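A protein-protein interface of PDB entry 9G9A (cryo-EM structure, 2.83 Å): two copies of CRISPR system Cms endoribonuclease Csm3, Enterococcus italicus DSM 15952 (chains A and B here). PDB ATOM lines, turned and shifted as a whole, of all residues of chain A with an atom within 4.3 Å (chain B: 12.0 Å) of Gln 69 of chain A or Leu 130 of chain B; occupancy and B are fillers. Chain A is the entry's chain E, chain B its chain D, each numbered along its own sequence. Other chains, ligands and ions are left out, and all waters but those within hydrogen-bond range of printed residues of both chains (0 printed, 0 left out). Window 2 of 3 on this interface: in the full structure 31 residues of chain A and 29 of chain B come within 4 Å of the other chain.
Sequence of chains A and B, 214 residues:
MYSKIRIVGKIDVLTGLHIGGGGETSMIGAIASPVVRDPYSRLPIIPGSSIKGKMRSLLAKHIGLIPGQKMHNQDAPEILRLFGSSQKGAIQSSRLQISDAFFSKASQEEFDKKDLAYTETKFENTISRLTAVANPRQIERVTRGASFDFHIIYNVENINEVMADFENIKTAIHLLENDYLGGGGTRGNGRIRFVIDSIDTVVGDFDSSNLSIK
No position is printed for both chains.
Of the 6 pairs that touch across the chains among the printed residues, none has its exchanged pair printed and touching as well.
Among the printed residues, merely in contact across the chains: Leu 65 of chain A with Arg 129 of chain B (3.6 Å), Gln 69 of chain A with Arg 129 of chain B (3.5 Å), Gln 69 of chain A with Leu 130 of chain B (3.3 Å), Lys 70 of chain A with Leu 130 of chain B (3.9 Å) and Met 71 of chain A with Arg 129 of chain B (3.7 Å).
Hydrophobic or aromatic side chains of chain A within 4 Å of the printed part of chain B: Leu 65.
The guanidinium group (NE) of Arg 129 of chain B is in salt-bridge range of the side-chain carboxylate (OD1) of Asp 75 of chain A, at 3.4 Å.
The backbone NH (N) of Ile 66 of chain A is in hydrogen-bond range of the side-chain amide oxygen (OE1) of Gln 69 of chain A (3.2 Å).
O of Met 71 of chain A sits at hydrogen-bond distance from NE2 of Gln 69 of chain A.
The side-chain carboxylate of Asp 75 of chain A sits at hydrogen-bond distance from the side-chain amide nitrogen of Gln 69 of chain A (2.4 Å).
Gln 69 of chain A touches just these residues of chain B: Arg 129 (3.5 Å) and Leu 130 (3.3 Å).
Of the printed residues of chain A, Leu 130 of chain B touches Gln 69 (3.3 Å) and Lys 70 (3.9 Å).
Leu 65 of chain A touches just one residue of chain B: Arg 129.
No residue of chain B comes within 4 Å of Ile 66 of chain A.
Of the printed residues of chain B, Lys 70 of chain A touches Leu 130 (3.9 Å).
No residue of chain B comes within 4 Å of Gln 74 of chain A.
Of the printed residues of chain A, Arg 129 of chain B touches Leu 65, Gln 69, Met 71 and Asp 75.
Of the printed residues of chain B, Met 71 of chain A touches Arg 129 (3.7 Å).
Ala 134 of chain B touches none of the printed residues of chain A.
Ser 128 of chain B touches none of the printed residues of chain A.
The nearest residue of chain B that does not touch Gln 69 of chain A is Thr 131 of chain B (5.9 Å).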
ATOM      1  N   LEU A  65      -9.013  -4.548 -30.274  1.00  0.00           N
ATOM      2  CA  LEU A  65      -8.762  -3.802 -29.050  1.00  0.00           C
ATOM      3  C   LEU A  65      -9.155  -4.622 -27.827  1.00  0.00           C
ATOM      4  O   LEU A  65     -10.125  -5.386 -27.855  1.00  0.00           O
ATOM      5  CB  LEU A  65      -9.534  -2.484 -29.064  1.00  0.00           C
ATOM      6  CG  LEU A  65      -9.122  -1.462 -30.123  1.00  0.00           C
ATOM      7  CD1 LEU A  65     -10.019  -0.238 -30.063  1.00  0.00           C
ATOM      8  CD2 LEU A  65      -7.670  -1.072 -29.938  1.00  0.00           C
ATOM      9  N   ILE A  66      -8.389  -4.463 -26.752  1.00  0.00           N
ATOM     10  CA  ILE A  66      -8.771  -5.072 -25.474  1.00  0.00           C
ATOM     11  C   ILE A  66     -10.078  -4.447 -25.002  1.00  0.00           C
ATOM     12  O   ILE A  66     -10.240  -3.215 -25.095  1.00  0.00           O
ATOM     13  CB  ILE A  66      -7.655  -4.877 -24.431  1.00  0.00           C
ATOM     14  CG1 ILE A  66      -6.419  -5.693 -24.811  1.00  0.00           C
ATOM     15  CG2 ILE A  66      -8.140  -5.250 -23.038  1.00  0.00           C
ATOM     16  CD1 ILE A  66      -5.324  -5.668 -23.766  1.00  0.00           C
ATOM     17  N   PRO A  67     -11.047  -5.228 -24.527  1.00  0.00           N
ATOM     18  CA  PRO A  67     -12.293  -4.633 -24.028  1.00  0.00           C
ATOM     19  C   PRO A  67     -12.022  -3.647 -22.901  1.00  0.00           C
ATOM     20  O   PRO A  67     -11.241  -3.921 -21.985  1.00  0.00           O
ATOM     21  CB  PRO A  67     -13.095  -5.845 -23.543  1.00  0.00           C
ATOM     22  CG  PRO A  67     -12.558  -6.988 -24.343  1.00  0.00           C
ATOM     23  CD  PRO A  67     -11.097  -6.701 -24.526  1.00  0.00           C
ATOM     24  N   GLY A  68     -12.678  -2.491 -22.973  1.00  0.00           N
ATOM     25  CA  GLY A  68     -12.467  -1.453 -21.985  1.00  0.00           C
ATOM     26  C   GLY A  68     -11.112  -0.788 -22.038  1.00  0.00           C
ATOM     27  O   GLY A  68     -10.688  -0.191 -21.047  1.00  0.00           O
ATOM     28  N   GLN A  69     -10.415  -0.877 -23.170  1.00  0.00           N
ATOM     29  CA  GLN A  69      -9.099  -0.264 -23.288  1.00  0.00           C
ATOM     30  C   GLN A  69      -9.211   1.254 -23.263  1.00  0.00           C
ATOM     31  O   GLN A  69     -10.079   1.837 -23.916  1.00  0.00           O
ATOM     32  CB  GLN A  69      -8.416  -0.722 -24.577  1.00  0.00           C
ATOM     33  CG  GLN A  69      -7.042  -0.113 -24.801  1.00  0.00           C
ATOM     34  CD  GLN A  69      -6.363  -0.644 -26.047  1.00  0.00           C
ATOM     35  OE1 GLN A  69      -6.778  -1.655 -26.611  1.00  0.00           O
ATOM     36  NE2 GLN A  69      -5.315   0.042 -26.486  1.00  0.00           N
ATOM     37  N   LYS A  70      -8.323   1.894 -22.500  1.00  0.00           N
ATOM     38  CA  LYS A  70      -8.283   3.346 -22.413  1.00  0.00           C
ATOM     39  C   LYS A  70      -6.893   3.933 -22.602  1.00  0.00           C
ATOM     40  O   LYS A  70      -6.737   5.151 -22.455  1.00  0.00           O
ATOM     41  CB  LYS A  70      -8.841   3.821 -21.061  1.00  0.00           C
ATOM     42  CG  LYS A  70      -7.934   3.532 -19.879  1.00  0.00           C
ATOM     43  CD  LYS A  70      -8.589   3.944 -18.571  1.00  0.00           C
ATOM     44  CE  LYS A  70      -9.091   5.378 -18.627  1.00  0.00           C
ATOM     45  NZ  LYS A  70      -8.000   6.348 -18.916  1.00  0.00           N
ATOM     46  N   MET A  71      -5.887   3.122 -22.914  1.00  0.00           N
ATOM     47  CA  MET A  71      -4.532   3.597 -23.138  1.00  0.00           C
ATOM     48  C   MET A  71      -3.999   3.011 -24.438  1.00  0.00           C
ATOM     49  O   MET A  71      -4.433   1.950 -24.890  1.00  0.00           O
ATOM     50  CB  MET A  71      -3.601   3.222 -21.973  1.00  0.00           C
ATOM     51  CG  MET A  71      -4.002   3.816 -20.633  1.00  0.00           C
ATOM     52  SD  MET A  71      -3.888   5.615 -20.607  1.00  0.00           S
ATOM     53  CE  MET A  71      -2.141   5.843 -20.929  1.00  0.00           C
ATOM     54  N   GLN A  74      -1.941  -0.357 -24.063  1.00  0.00           N
ATOM     55  CA  GLN A  74      -2.677  -1.593 -23.843  1.00  0.00           C
ATOM     56  C   GLN A  74      -2.995  -2.314 -25.148  1.00  0.00           C
ATOM     57  O   GLN A  74      -3.927  -3.122 -25.192  1.00  0.00           O
ATOM     58  CB  GLN A  74      -3.967  -1.310 -23.072  1.00  0.00           C
ATOM     59  CG  GLN A  74      -3.760  -0.612 -21.739  1.00  0.00           C
ATOM     60  CD  GLN A  74      -5.065  -0.367 -21.007  1.00  0.00           C
ATOM     61  OE1 GLN A  74      -6.122  -0.841 -21.426  1.00  0.00           O
ATOM     62  NE2 GLN A  74      -5.000   0.376 -19.909  1.00  0.00           N
ATOM     63  N   ASP A  75      -2.247  -2.033 -26.211  1.00  0.00           N
ATOM     64  CA  ASP A  75      -2.486  -2.662 -27.500  1.00  0.00           C
ATOM     65  C   ASP A  75      -1.807  -4.029 -27.555  1.00  0.00           C
ATOM     66  O   ASP A  75      -1.240  -4.516 -26.572  1.00  0.00           O
ATOM     67  CB  ASP A  75      -2.001  -1.756 -28.630  1.00  0.00           C
ATOM     68  CG  ASP A  75      -2.821  -0.484 -28.753  1.00  0.00           C
ATOM     69  OD1 ASP A  75      -4.027  -0.515 -28.433  1.00  0.00           O
ATOM     70  OD2 ASP A  75      -2.259   0.549 -29.171  1.00  0.00           O
ATOM     71  N   THR B 126      -4.314  13.432 -29.485  1.00  0.00           N
ATOM     72  CA  THR B 126      -4.345  12.007 -29.187  1.00  0.00           C
ATOM     73  C   THR B 126      -5.790  11.539 -29.206  1.00  0.00           C
ATOM     74  O   THR B 126      -6.629  12.075 -28.476  1.00  0.00           O
ATOM     75  CB  THR B 126      -3.714  11.714 -27.823  1.00  0.00           C
ATOM     76  OG1 THR B 126      -2.442  12.365 -27.733  1.00  0.00           O
ATOM     77  CG2 THR B 126      -3.525  10.218 -27.631  1.00  0.00           C
ATOM     78  N   ILE B 127      -6.080  10.543 -30.035  1.00  0.00           N
ATOM     79  CA  ILE B 127      -7.410   9.951 -30.090  1.00  0.00           C
ATOM     80  C   ILE B 127      -7.444   8.794 -29.103  1.00  0.00           C
ATOM     81  O   ILE B 127      -6.731   7.798 -29.274  1.00  0.00           O
ATOM     82  CB  ILE B 127      -7.765   9.486 -31.512  1.00  0.00           C
ATOM     83  CG1 ILE B 127      -8.161  10.675 -32.394  1.00  0.00           C
ATOM     84  CG2 ILE B 127      -8.901   8.477 -31.478  1.00  0.00           C
ATOM     85  CD1 ILE B 127      -7.001  11.486 -32.925  1.00  0.00           C
ATOM     86  N   SER B 128      -8.260   8.932 -28.062  1.00  0.00           N
ATOM     87  CA  SER B 128      -8.307   7.928 -27.009  1.00  0.00           C
ATOM     88  C   SER B 128      -8.868   6.614 -27.538  1.00  0.00           C
ATOM     89  O   SER B 128      -9.763   6.595 -28.387  1.00  0.00           O
ATOM     90  CB  SER B 128      -9.154   8.429 -25.839  1.00  0.00           C
ATOM     91  OG  SER B 128     -10.484   8.693 -26.244  1.00  0.00           O
ATOM     92  N   ARG B 129      -8.330   5.506 -27.026  1.00  0.00           N
ATOM     93  CA  ARG B 129      -8.839   4.187 -27.374  1.00  0.00           C
ATOM     94  C   ARG B 129     -10.217   3.915 -26.790  1.00  0.00           C
ATOM     95  O   ARG B 129     -10.857   2.937 -27.192  1.00  0.00           O
ATOM     96  CB  ARG B 129      -7.864   3.109 -26.903  1.00  0.00           C
ATOM     97  CG  ARG B 129      -6.579   3.036 -27.703  1.00  0.00           C
ATOM     98  CD  ARG B 129      -6.795   2.332 -29.032  1.00  0.00           C
ATOM     99  NE  ARG B 129      -5.549   2.191 -29.777  1.00  0.00           N
ATOM    100  CZ  ARG B 129      -5.177   2.987 -30.769  1.00  0.00           C
ATOM    101  NH1 ARG B 129      -5.948   3.977 -31.186  1.00  0.00           N
ATOM    102  NH2 ARG B 129      -4.002   2.784 -31.357  1.00  0.00           N
ATOM    103  N   LEU B 130     -10.687   4.745 -25.859  1.00  0.00           N
ATOM    104  CA  LEU B 130     -11.956   4.516 -25.179  1.00  0.00           C
ATOM    105  C   LEU B 130     -13.056   5.435 -25.690  1.00  0.00           C
ATOM    106  O   LEU B 130     -14.126   4.953 -26.071  1.00  0.00           O
ATOM    107  CB  LEU B 130     -11.769   4.689 -23.664  1.00  0.00           C
ATOM    108  CG  LEU B 130     -13.016   4.538 -22.792  1.00  0.00           C
ATOM    109  CD1 LEU B 130     -13.546   3.114 -22.852  1.00  0.00           C
ATOM    110  CD2 LEU B 130     -12.723   4.946 -21.358  1.00  0.00           C
ATOM    111  N   THR B 131     -12.824   6.746 -25.712  1.00  0.00           N
ATOM    112  CA  THR B 131     -13.850   7.707 -26.090  1.00  0.00           C
ATOM    113  C   THR B 131     -13.685   8.247 -27.503  1.00  0.00           C
ATOM    114  O   THR B 131     -14.622   8.865 -28.021  1.00  0.00           O
ATOM    115  CB  THR B 131     -13.858   8.881 -25.106  1.00  0.00           C
ATOM    116  OG1 THR B 131     -12.566   9.500 -25.086  1.00  0.00           O
ATOM    117  CG2 THR B 131     -14.202   8.397 -23.709  1.00  0.00           C
ATOM    118  N   ALA B 132     -12.523   8.047 -28.127  1.00  0.00           N
ATOM    119  CA  ALA B 132     -12.156   8.557 -29.445  1.00  0.00           C
ATOM    120  C   ALA B 132     -12.027  10.075 -29.469  1.00  0.00           C
ATOM    121  O   ALA B 132     -11.810  10.645 -30.544  1.00  0.00           O
ATOM    122  CB  ALA B 132     -13.134   8.119 -30.546  1.00  0.00           C
ATOM    123  N   VAL B 133     -12.148  10.749 -28.324  1.00  0.00           N
ATOM    124  CA  VAL B 133     -12.021  12.199 -28.280  1.00  0.00           C
ATOM    125  C   VAL B 133     -10.563  12.595 -28.471  1.00  0.00           C
ATOM    126  O   VAL B 133      -9.655  12.012 -27.863  1.00  0.00           O
ATOM    127  CB  VAL B 133     -12.576  12.741 -26.952  1.00  0.00           C
ATOM    128  CG1 VAL B 133     -12.319  14.235 -26.832  1.00  0.00           C
ATOM    129  CG2 VAL B 133     -14.064  12.446 -26.843  1.00  0.00           C
ATOM    130  N   ALA B 134     -10.333  13.594 -29.316  1.00  0.00           N
ATOM    131  CA  ALA B 134      -8.998  14.112 -29.571  1.00  0.00           C
ATOM    132  C   ALA B 134      -8.583  15.045 -28.443  1.00  0.00           C
ATOM    133  O   ALA B 134      -9.377  15.868 -27.979  1.00  0.00           O
ATOM    134  CB  ALA B 134      -8.943  14.853 -30.907  1.00  0.00           C
ATOM    135  N   ASN B 135      -7.334  14.911 -28.005  1.00  0.00           N
ATOM    136  CA  ASN B 135      -6.796  15.739 -26.937  1.00  0.00           C
ATOM    137  C   ASN B 135      -5.754  16.682 -27.513  1.00  0.00           C
ATOM    138  O   ASN B 135      -4.623  16.253 -27.783  1.00  0.00           O
ATOM    139  CB  ASN B 135      -6.186  14.875 -25.836  1.00  0.00           C
ATOM    140  CG  ASN B 135      -5.742  15.689 -24.641  1.00  0.00           C
ATOM    141  OD1 ASN B 135      -4.588  16.108 -24.554  1.00  0.00           O
ATOM    142  ND2 ASN B 135      -6.659  15.921 -23.710  1.00  0.00           N
